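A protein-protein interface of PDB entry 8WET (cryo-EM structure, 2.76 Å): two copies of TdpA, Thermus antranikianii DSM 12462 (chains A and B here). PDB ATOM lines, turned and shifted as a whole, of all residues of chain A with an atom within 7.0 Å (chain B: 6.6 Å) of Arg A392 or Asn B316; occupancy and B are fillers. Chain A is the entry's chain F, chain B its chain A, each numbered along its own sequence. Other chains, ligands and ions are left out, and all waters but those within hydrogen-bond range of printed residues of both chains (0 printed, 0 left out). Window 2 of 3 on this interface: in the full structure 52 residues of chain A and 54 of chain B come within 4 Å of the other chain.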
ATOM      1  N   TYR A 313     -25.960  13.487  20.840  1.00  0.00           N
ATOM      2  CA  TYR A 313     -26.382  14.110  19.589  1.00  0.00           C
ATOM      3  C   TYR A 313     -27.734  14.796  19.747  1.00  0.00           C
ATOM      4  O   TYR A 313     -27.951  15.886  19.204  1.00  0.00           O
ATOM      5  CB  TYR A 313     -26.418  13.075  18.461  1.00  0.00           C
ATOM      6  CG  TYR A 313     -27.494  12.019  18.586  1.00  0.00           C
ATOM      7  CD1 TYR A 313     -27.270  10.850  19.300  1.00  0.00           C
ATOM      8  CD2 TYR A 313     -28.730  12.183  17.975  1.00  0.00           C
ATOM      9  CE1 TYR A 313     -28.249   9.880  19.408  1.00  0.00           C
ATOM     10  CE2 TYR A 313     -29.715  11.221  18.081  1.00  0.00           C
ATOM     11  CZ  TYR A 313     -29.470  10.072  18.799  1.00  0.00           C
ATOM     12  OH  TYR A 313     -30.448   9.111  18.906  1.00  0.00           O
ATOM     13  N   ALA A 337     -33.643  13.078   8.143  1.00  0.00           N
ATOM     14  CA  ALA A 337     -33.955  12.245   9.300  1.00  0.00           C
ATOM     15  C   ALA A 337     -35.458  12.143   9.511  1.00  0.00           C
ATOM     16  O   ALA A 337     -35.987  11.055   9.774  1.00  0.00           O
ATOM     17  CB  ALA A 337     -33.272  12.802  10.549  1.00  0.00           C
ATOM     18  N   LYS A 340     -36.800   9.822   6.773  1.00  0.00           N
ATOM     19  CA  LYS A 340     -36.479   8.426   7.050  1.00  0.00           C
ATOM     20  C   LYS A 340     -37.283   7.889   8.225  1.00  0.00           C
ATOM     21  O   LYS A 340     -37.507   6.676   8.316  1.00  0.00           O
ATOM     22  CB  LYS A 340     -34.983   8.271   7.320  1.00  0.00           C
ATOM     23  CG  LYS A 340     -34.177   7.804   6.121  1.00  0.00           C
ATOM     24  CD  LYS A 340     -32.690   7.800   6.428  1.00  0.00           C
ATOM     25  CE  LYS A 340     -32.366   6.866   7.582  1.00  0.00           C
ATOM     26  NZ  LYS A 340     -30.902   6.793   7.842  1.00  0.00           N
ATOM     27  N   LYS A 383     -18.283  12.837  13.168  1.00  0.00           N
ATOM     28  CA  LYS A 383     -19.699  12.478  13.100  1.00  0.00           C
ATOM     29  C   LYS A 383     -20.463  13.370  14.076  1.00  0.00           C
ATOM     30  O   LYS A 383     -20.709  13.025  15.235  1.00  0.00           O
ATOM     31  CB  LYS A 383     -19.892  10.998  13.409  1.00  0.00           C
ATOM     32  CG  LYS A 383     -18.936  10.089  12.649  1.00  0.00           C
ATOM     33  CD  LYS A 383     -19.161   8.625  12.989  1.00  0.00           C
ATOM     34  CE  LYS A 383     -18.447   7.717  12.001  1.00  0.00           C
ATOM     35  NZ  LYS A 383     -18.536   6.283  12.393  1.00  0.00           N
ATOM     36  N   ALA A 386     -25.740  16.600  13.276  1.00  0.00           N
ATOM     37  CA  ALA A 386     -26.650  16.420  12.148  1.00  0.00           C
ATOM     38  C   ALA A 386     -26.499  15.037  11.525  1.00  0.00           C
ATOM     39  O   ALA A 386     -27.494  14.353  11.252  1.00  0.00           O
ATOM     40  CB  ALA A 386     -26.413  17.512  11.106  1.00  0.00           C
ATOM     41  N   ARG A 387     -25.258  14.607  11.286  1.00  0.00           N
ATOM     42  CA  ARG A 387     -25.040  13.294  10.688  1.00  0.00           C
ATOM     43  C   ARG A 387     -25.479  12.179  11.629  1.00  0.00           C
ATOM     44  O   ARG A 387     -26.043  11.169  11.191  1.00  0.00           O
ATOM     45  CB  ARG A 387     -23.570  13.134  10.299  1.00  0.00           C
ATOM     46  CG  ARG A 387     -23.329  12.095   9.218  1.00  0.00           C
ATOM     47  CD  ARG A 387     -21.846  11.897   8.957  1.00  0.00           C
ATOM     48  NE  ARG A 387     -21.237  13.075   8.349  1.00  0.00           N
ATOM     49  CZ  ARG A 387     -20.123  13.649   8.779  1.00  0.00           C
ATOM     50  NH1 ARG A 387     -19.460  13.179   9.822  1.00  0.00           N
ATOM     51  NH2 ARG A 387     -19.662  14.724   8.145  1.00  0.00           N
ATOM     52  N   GLU A 388     -25.236  12.346  12.931  1.00  0.00           N
ATOM     53  CA  GLU A 388     -25.689  11.344  13.891  1.00  0.00           C
ATOM     54  C   GLU A 388     -27.211  11.296  13.973  1.00  0.00           C
ATOM     55  O   GLU A 388     -27.782  10.216  14.148  1.00  0.00           O
ATOM     56  CB  GLU A 388     -25.082  11.618  15.266  1.00  0.00           C
ATOM     57  CG  GLU A 388     -24.915  10.375  16.122  1.00  0.00           C
ATOM     58  CD  GLU A 388     -23.902  10.567  17.233  1.00  0.00           C
ATOM     59  OE1 GLU A 388     -23.327  11.670  17.330  1.00  0.00           O
ATOM     60  OE2 GLU A 388     -23.680   9.612  18.008  1.00  0.00           O
ATOM     61  N   LEU A 389     -27.882  12.444  13.849  1.00  0.00           N
ATOM     62  CA  LEU A 389     -29.339  12.440  13.756  1.00  0.00           C
ATOM     63  C   LEU A 389     -29.807  11.703  12.511  1.00  0.00           C
ATOM     64  O   LEU A 389     -30.776  10.938  12.560  1.00  0.00           O
ATOM     65  CB  LEU A 389     -29.878  13.869  13.744  1.00  0.00           C
ATOM     66  CG  LEU A 389     -30.005  14.630  15.059  1.00  0.00           C
ATOM     67  CD1 LEU A 389     -30.402  16.057  14.758  1.00  0.00           C
ATOM     68  CD2 LEU A 389     -31.031  13.967  15.957  1.00  0.00           C
ATOM     69  N   TYR A 390     -29.147  11.939  11.377  1.00  0.00           N
ATOM     70  CA  TYR A 390     -29.525  11.230  10.160  1.00  0.00           C
ATOM     71  C   TYR A 390     -29.345   9.728  10.329  1.00  0.00           C
ATOM     72  O   TYR A 390     -30.149   8.935   9.824  1.00  0.00           O
ATOM     73  CB  TYR A 390     -28.711  11.743   8.973  1.00  0.00           C
ATOM     74  CG  TYR A 390     -29.091  11.092   7.663  1.00  0.00           C
ATOM     75  CD1 TYR A 390     -30.281  11.414   7.027  1.00  0.00           C
ATOM     76  CD2 TYR A 390     -28.262  10.155   7.065  1.00  0.00           C
ATOM     77  CE1 TYR A 390     -30.635  10.822   5.833  1.00  0.00           C
ATOM     78  CE2 TYR A 390     -28.606   9.558   5.870  1.00  0.00           C
ATOM     79  CZ  TYR A 390     -29.794   9.895   5.259  1.00  0.00           C
ATOM     80  OH  TYR A 390     -30.141   9.301   4.067  1.00  0.00           O
ATOM     81  N   SER A 391     -28.295   9.319  11.042  1.00  0.00           N
ATOM     82  CA  SER A 391     -28.071   7.896  11.282  1.00  0.00           C
ATOM     83  C   SER A 391     -29.119   7.310  12.223  1.00  0.00           C
ATOM     84  O   SER A 391     -29.625   6.208  11.985  1.00  0.00           O
ATOM     85  CB  SER A 391     -26.663   7.677  11.838  1.00  0.00           C
ATOM     86  OG  SER A 391     -26.581   8.074  13.195  1.00  0.00           O
ATOM     87  N   ARG A 392     -29.460   8.027  13.297  1.00  0.00           N
ATOM     88  CA  ARG A 392     -30.365   7.530  14.328  1.00  0.00           C
ATOM     89  C   ARG A 392     -31.782   8.077  14.180  1.00  0.00           C
ATOM     90  O   ARG A 392     -32.515   8.177  15.169  1.00  0.00           O
ATOM     91  CB  ARG A 392     -29.814   7.857  15.715  1.00  0.00           C
ATOM     92  CG  ARG A 392     -28.356   7.477  15.913  1.00  0.00           C
ATOM     93  CD  ARG A 392     -28.104   6.029  15.525  1.00  0.00           C
ATOM     94  NE  ARG A 392     -26.697   5.664  15.631  1.00  0.00           N
ATOM     95  CZ  ARG A 392     -26.080   5.378  16.769  1.00  0.00           C
ATOM     96  NH1 ARG A 392     -26.718   5.404  17.927  1.00  0.00           N
ATOM     97  NH2 ARG A 392     -24.790   5.058  16.744  1.00  0.00           N
ATOM     98  N   ALA A 393     -32.175   8.443  12.960  1.00  0.00           N
ATOM     99  CA  ALA A 393     -33.518   8.930  12.652  1.00  0.00           C
ATOM    100  C   ALA A 393     -34.650   8.045  13.164  1.00  0.00           C
ATOM    101  O   ALA A 393     -35.807   8.476  13.182  1.00  0.00           O
ATOM    102  CB  ALA A 393     -33.666   9.102  11.139  1.00  0.00           C
ATOM    103  N   LYS A 394     -34.344   6.812  13.571  1.00  0.00           N
ATOM    104  CA  LYS A 394     -35.376   5.935  14.111  1.00  0.00           C
ATOM    105  C   LYS A 394     -36.025   6.507  15.366  1.00  0.00           C
ATOM    106  O   LYS A 394     -37.141   6.106  15.711  1.00  0.00           O
ATOM    107  CB  LYS A 394     -34.788   4.554  14.411  1.00  0.00           C
ATOM    108  CG  LYS A 394     -35.826   3.461  14.601  1.00  0.00           C
ATOM    109  CD  LYS A 394     -35.182   2.141  14.980  1.00  0.00           C
ATOM    110  CE  LYS A 394     -34.750   2.138  16.436  1.00  0.00           C
ATOM    111  NZ  LYS A 394     -34.385   0.774  16.901  1.00  0.00           N
ATOM    112  N   VAL A 395     -35.359   7.443  16.049  1.00  0.00           N
ATOM    113  CA  VAL A 395     -35.915   8.046  17.256  1.00  0.00           C
ATOM    114  C   VAL A 395     -37.131   8.917  16.984  1.00  0.00           C
ATOM    115  O   VAL A 395     -37.824   9.305  17.932  1.00  0.00           O
ATOM    116  CB  VAL A 395     -34.845   8.883  17.985  1.00  0.00           C
ATOM    117  CG1 VAL A 395     -33.644   8.023  18.332  1.00  0.00           C
ATOM    118  CG2 VAL A 395     -34.428  10.070  17.133  1.00  0.00           C
ATOM    119  N   PHE A 396     -37.410   9.238  15.722  1.00  0.00           N
ATOM    120  CA  PHE A 396     -38.548  10.069  15.354  1.00  0.00           C
ATOM    121  C   PHE A 396     -39.737   9.254  14.863  1.00  0.00           C
ATOM    122  O   PHE A 396     -40.687   9.826  14.322  1.00  0.00           O
ATOM    123  CB  PHE A 396     -38.139  11.076  14.277  1.00  0.00           C
ATOM    124  CG  PHE A 396     -37.231  12.162  14.769  1.00  0.00           C
ATOM    125  CD1 PHE A 396     -37.611  12.982  15.814  1.00  0.00           C
ATOM    126  CD2 PHE A 396     -35.997  12.367  14.180  1.00  0.00           C
ATOM    127  CE1 PHE A 396     -36.776  13.983  16.265  1.00  0.00           C
ATOM    128  CE2 PHE A 396     -35.159  13.366  14.627  1.00  0.00           C
ATOM    129  CZ  PHE A 396     -35.551  14.176  15.672  1.00  0.00           C
ATOM    130  N   TYR B 300     -29.144  -6.345  22.117  1.00  0.00           N
ATOM    131  CA  TYR B 300     -28.823  -4.956  22.427  1.00  0.00           C
ATOM    132  C   TYR B 300     -29.135  -4.606  23.876  1.00  0.00           C
ATOM    133  O   TYR B 300     -28.478  -3.735  24.455  1.00  0.00           O
ATOM    134  CB  TYR B 300     -29.583  -4.024  21.484  1.00  0.00           C
ATOM    135  CG  TYR B 300     -29.315  -2.556  21.711  1.00  0.00           C
ATOM    136  CD1 TYR B 300     -28.054  -2.020  21.495  1.00  0.00           C
ATOM    137  CD2 TYR B 300     -30.325  -1.702  22.134  1.00  0.00           C
ATOM    138  CE1 TYR B 300     -27.804  -0.679  21.699  1.00  0.00           C
ATOM    139  CE2 TYR B 300     -30.085  -0.358  22.338  1.00  0.00           C
ATOM    140  CZ  TYR B 300     -28.823   0.148  22.119  1.00  0.00           C
ATOM    141  OH  TYR B 300     -28.577   1.486  22.322  1.00  0.00           O
ATOM    142  N   PRO B 311     -21.990  -1.901  23.038  1.00  0.00           N
ATOM    143  CA  PRO B 311     -20.997  -1.782  21.966  1.00  0.00           C
ATOM    144  C   PRO B 311     -21.538  -0.992  20.785  1.00  0.00           C
ATOM    145  O   PRO B 311     -22.733  -1.015  20.485  1.00  0.00           O
ATOM    146  CB  PRO B 311     -20.704  -3.237  21.585  1.00  0.00           C
ATOM    147  CG  PRO B 311     -21.877  -4.011  22.073  1.00  0.00           C
ATOM    148  CD  PRO B 311     -22.380  -3.298  23.287  1.00  0.00           C
ATOM    149  N   GLN B 312     -20.630  -0.279  20.115  1.00  0.00           N
ATOM    150  CA  GLN B 312     -21.035   0.612  19.033  1.00  0.00           C
ATOM    151  C   GLN B 312     -21.581  -0.165  17.840  1.00  0.00           C
ATOM    152  O   GLN B 312     -22.510   0.297  17.167  1.00  0.00           O
ATOM    153  CB  GLN B 312     -19.857   1.490  18.610  1.00  0.00           C
ATOM    154  CG  GLN B 312     -20.220   2.581  17.616  1.00  0.00           C
ATOM    155  CD  GLN B 312     -21.218   3.574  18.177  1.00  0.00           C
ATOM    156  OE1 GLN B 312     -22.128   4.018  17.478  1.00  0.00           O
ATOM    157  NE2 GLN B 312     -21.050   3.929  19.446  1.00  0.00           N
ATOM    158  N   TYR B 313     -21.019  -1.343  17.560  1.00  0.00           N
ATOM    159  CA  TYR B 313     -21.469  -2.103  16.399  1.00  0.00           C
ATOM    160  C   TYR B 313     -22.884  -2.636  16.585  1.00  0.00           C
ATOM    161  O   TYR B 313     -23.596  -2.850  15.597  1.00  0.00           O
ATOM    162  CB  TYR B 313     -20.496  -3.245  16.101  1.00  0.00           C
ATOM    163  CG  TYR B 313     -20.631  -4.452  17.000  1.00  0.00           C
ATOM    164  CD1 TYR B 313     -20.132  -4.438  18.294  1.00  0.00           C
ATOM    165  CD2 TYR B 313     -21.244  -5.612  16.549  1.00  0.00           C
ATOM    166  CE1 TYR B 313     -20.248  -5.544  19.114  1.00  0.00           C
ATOM    167  CE2 TYR B 313     -21.365  -6.720  17.363  1.00  0.00           C
ATOM    168  CZ  TYR B 313     -20.866  -6.679  18.645  1.00  0.00           C
ATOM    169  OH  TYR B 313     -20.982  -7.779  19.462  1.00  0.00           O
ATOM    170  N   LEU B 314     -23.308  -2.861  17.829  1.00  0.00           N
ATOM    171  CA  LEU B 314     -24.692  -3.243  18.077  1.00  0.00           C
ATOM    172  C   LEU B 314     -25.635  -2.053  17.969  1.00  0.00           C
ATOM    173  O   LEU B 314     -26.788  -2.218  17.556  1.00  0.00           O
ATOM    174  CB  LEU B 314     -24.824  -3.895  19.454  1.00  0.00           C
ATOM    175  CG  LEU B 314     -24.688  -5.418  19.493  1.00  0.00           C
ATOM    176  CD1 LEU B 314     -24.944  -5.940  20.895  1.00  0.00           C
ATOM    177  CD2 LEU B 314     -25.628  -6.072  18.494  1.00  0.00           C
ATOM    178  N   GLU B 315     -25.171  -0.858  18.341  1.00  0.00           N
ATOM    179  CA  GLU B 315     -25.998   0.337  18.206  1.00  0.00           C
ATOM    180  C   GLU B 315     -26.289   0.642  16.743  1.00  0.00           C
ATOM    181  O   GLU B 315     -27.409   1.037  16.393  1.00  0.00           O
ATOM    182  CB  GLU B 315     -25.314   1.527  18.875  1.00  0.00           C
ATOM    183  CG  GLU B 315     -25.788   1.802  20.291  1.00  0.00           C
ATOM    184  CD  GLU B 315     -25.256   3.110  20.841  1.00  0.00           C
ATOM    185  OE1 GLU B 315     -24.516   3.806  20.115  1.00  0.00           O
ATOM    186  OE2 GLU B 315     -25.576   3.441  22.002  1.00  0.00           O
ATOM    187  N   ASN B 316     -25.290   0.480  15.872  1.00  0.00           N
ATOM    188  CA  ASN B 316     -25.503   0.709  14.447  1.00  0.00           C
ATOM    189  C   ASN B 316     -26.517  -0.274  13.877  1.00  0.00           C
ATOM    190  O   ASN B 316     -27.389   0.107  13.090  1.00  0.00           O
ATOM    191  CB  ASN B 316     -24.177   0.608  13.695  1.00  0.00           C
ATOM    192  CG  ASN B 316     -23.113   1.524  14.264  1.00  0.00           C
ATOM    193  OD1 ASN B 316     -23.404   2.641  14.692  1.00  0.00           O
ATOM    194  ND2 ASN B 316     -21.871   1.056  14.271  1.00  0.00           N
ATOM    195  N   ALA B 317     -26.412  -1.548  14.261  1.00  0.00           N
ATOM    196  CA  ALA B 317     -27.362  -2.547  13.783  1.00  0.00           C
ATOM    197  C   ALA B 317     -28.765  -2.273  14.305  1.00  0.00           C
ATOM    198  O   ALA B 317     -29.751  -2.476  13.588  1.00  0.00           O
ATOM    199  CB  ALA B 317     -26.902  -3.944  14.194  1.00  0.00           C
ATOM    200  N   PHE B 318     -28.873  -1.818  15.554  1.00  0.00           N
ATOM    201  CA  PHE B 318     -30.183  -1.574  16.149  1.00  0.00           C
ATOM    202  C   PHE B 318     -30.938  -0.478  15.405  1.00  0.00           C
ATOM    203  O   PHE B 318     -32.144  -0.600  15.164  1.00  0.00           O
ATOM    204  CB  PHE B 318     -30.022  -1.209  17.624  1.00  0.00           C
ATOM    205  CG  PHE B 318     -31.321  -1.053  18.359  1.00  0.00           C
ATOM    206  CD1 PHE B 318     -32.234  -2.091  18.408  1.00  0.00           C
ATOM    207  CD2 PHE B 318     -31.624   0.131  19.009  1.00  0.00           C
ATOM    208  CE1 PHE B 318     -33.429  -1.950  19.087  1.00  0.00           C
ATOM    209  CE2 PHE B 318     -32.817   0.279  19.689  1.00  0.00           C
ATOM    210  CZ  PHE B 318     -33.720  -0.763  19.729  1.00  0.00           C
ATOM    211  N   TYR B 319     -30.247   0.596  15.032  1.00  0.00           N
ATOM    212  CA  TYR B 319     -30.890   1.756  14.432  1.00  0.00           C
ATOM    213  C   TYR B 319     -30.944   1.711  12.910  1.00  0.00           C
ATOM    214  O   TYR B 319     -31.609   2.562  12.309  1.00  0.00           O
ATOM    215  CB  TYR B 319     -30.172   3.037  14.867  1.00  0.00           C
ATOM    216  CG  TYR B 319     -30.519   3.492  16.264  1.00  0.00           C
ATOM    217  CD1 TYR B 319     -31.660   4.241  16.507  1.00  0.00           C
ATOM    218  CD2 TYR B 319     -29.703   3.174  17.341  1.00  0.00           C
ATOM    219  CE1 TYR B 319     -31.981   4.660  17.783  1.00  0.00           C
ATOM    220  CE2 TYR B 319     -30.016   3.588  18.620  1.00  0.00           C
ATOM    221  CZ  TYR B 319     -31.156   4.331  18.835  1.00  0.00           C
ATOM    222  OH  TYR B 319     -31.472   4.746  20.107  1.00  0.00           O
ATOM    223  N   ASN B 320     -30.273   0.751  12.267  1.00  0.00           N
ATOM    224  CA  ASN B 320     -30.158   0.755  10.815  1.00  0.00           C
ATOM    225  C   ASN B 320     -30.402  -0.609  10.178  1.00  0.00           C
ATOM    226  O   ASN B 320     -30.079  -0.789   8.998  1.00  0.00           O
ATOM    227  CB  ASN B 320     -28.781   1.277  10.391  1.00  0.00           C
ATOM    228  CG  ASN B 320     -28.545   2.712  10.819  1.00  0.00           C
ATOM    229  OD1 ASN B 320     -27.540   3.025  11.458  1.00  0.00           O
ATOM    230  ND2 ASN B 320     -29.472   3.594  10.467  1.00  0.00           N
ATOM    231  N   LEU B 321     -30.962  -1.572  10.914  1.00  0.00           N
ATOM    232  CA  LEU B 321     -31.228  -2.879  10.322  1.00  0.00           C
ATOM    233  C   LEU B 321     -32.340  -2.813   9.283  1.00  0.00           C
ATOM    234  O   LEU B 321     -32.308  -3.558   8.297  1.00  0.00           O
ATOM    235  CB  LEU B 321     -31.579  -3.892  11.411  1.00  0.00           C
ATOM    236  CG  LEU B 321     -31.876  -5.319  10.944  1.00  0.00           C
ATOM    237  CD1 LEU B 321     -30.723  -5.867  10.121  1.00  0.00           C
ATOM    238  CD2 LEU B 321     -32.155  -6.216  12.134  1.00  0.00           C
ATOM    239  N   TRP B 324     -31.007  -1.961   5.943  1.00  0.00           N
ATOM    240  CA  TRP B 324     -30.219  -3.050   5.375  1.00  0.00           C
ATOM    241  C   TRP B 324     -31.086  -4.090   4.679  1.00  0.00           C
ATOM    242  O   TRP B 324     -30.581  -4.825   3.823  1.00  0.00           O
ATOM    243  CB  TRP B 324     -29.384  -3.729   6.462  1.00  0.00           C
ATOM    244  CG  TRP B 324     -28.397  -2.826   7.134  1.00  0.00           C
ATOM    245  CD1 TRP B 324     -28.070  -1.553   6.772  1.00  0.00           C
ATOM    246  CD2 TRP B 324     -27.609  -3.129   8.291  1.00  0.00           C
ATOM    247  NE1 TRP B 324     -27.127  -1.044   7.631  1.00  0.00           N
ATOM    248  CE2 TRP B 324     -26.828  -1.993   8.573  1.00  0.00           C
ATOM    249  CE3 TRP B 324     -27.490  -4.251   9.116  1.00  0.00           C
ATOM    250  CZ2 TRP B 324     -25.938  -1.947   9.644  1.00  0.00           C
ATOM    251  CZ3 TRP B 324     -26.607  -4.203  10.179  1.00  0.00           C
ATOM    252  CH2 TRP B 324     -25.843  -3.059  10.432  1.00  0.00           C
ATOM    253  N   GLY B 384     -18.010  -1.914   7.656  1.00  0.00           N
ATOM    254  CA  GLY B 384     -19.349  -1.412   7.861  1.00  0.00           C
ATOM    255  C   GLY B 384     -20.041  -2.039   9.055  1.00  0.00           C
ATOM    256  O   GLY B 384     -19.514  -2.915   9.740  1.00  0.00           O
ATOM    257  N   GLY B 385     -21.263  -1.565   9.302  1.00  0.00           N
ATOM    258  CA  GLY B 385     -22.040  -2.094  10.409  1.00  0.00           C
ATOM    259  C   GLY B 385     -22.430  -3.546  10.216  1.00  0.00           C
ATOM    260  O   GLY B 385     -22.393  -4.339  11.160  1.00  0.00           O
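Of the 15 printed residues of chain B, 6 touch a printed residue of chain A. Of the 15 printed residues of chain A, 4 touch a printed residue of chain B. Hydrophobic or aromatic side chains of chain A within 4 Å of the printed part of chain B: Val A395. Among the printed residues, Asp or Glu carboxylates within 4 Å of a Lys or Arg side-chain nitrogen of the other chain: Arg A392 with Glu B315 (3.5 Å).
Arg A392 touches Tyr B319. CD1 of Tyr B319 touches CE of Lys A394, 3.7 Å away. CG1 of Val A395 touches CE1 of Tyr B319, 3.8 Å away.
OE1 of Gln B312 is in hydrogen-bond range of NH2 of Arg A392. NH1 of Arg A392 is in salt-bridge range of OE1 of Glu B315. The side-chain amide oxygen (OD1) of Asn B316 sits at hydrogen-bond distance from the guanidinium group (NH2) of Arg A392. The backbone carbonyl oxygen (O) of Phe B318 lies within hydrogen-bond range of the side-chain amino group (NZ) of Lys A394 (3.2 Å). The backbone carbonyl oxygen of Ser A391 sits at hydrogen-bond distance from the side-chain amide nitrogen of Asn B320.
Position printed for both chains: 313. Of the 8 pairs that touch across the chains among the printed residues, none has its exchanged pair printed and touching as well.
Ala A386 touches none of the printed residues of chain B. Arg A392 touches just these residues of chain B: Gln B312 (3.0 Å), Glu B315 (3.5 Å), Asn B316 (3.5 Å) and Tyr B319 (3.6 Å). Printed residues of chain A within 4 Å of Gln B312: Arg A392. Of chain A, only Arg A392 comes within 4 Å of Asn B316. Of the printed residues of chain A, Tyr B319 touches Arg A392 (3.6 Å), Lys A394 (3.7 Å) and Val A395 (3.8 Å). The nearest printed residue of chain A that does not touch Asn B316 is Ser A391 (6.5 Å). The nearest printed residue of chain B that does not touch Val A395 is Phe B318 (7.9 Å).
The backbone carbonyl oxygen of Gln B312 lies within hydrogen-bond range of the side-chain amide nitrogen of Asn B316 (3.1 Å). The backbone carbonyl oxygen of Asn B316 sits close to the side-chain amide oxygen of Asn B320. O of Asn B320 sits close to NE1 of Trp B324. O of Glu A388 sits at hydrogen-bond distance from OG of Ser A391, 2.6 Å away. The side-chain hydroxyl of Ser A391 lies close to the guanidinium group of Arg A392 (3.4 Å).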
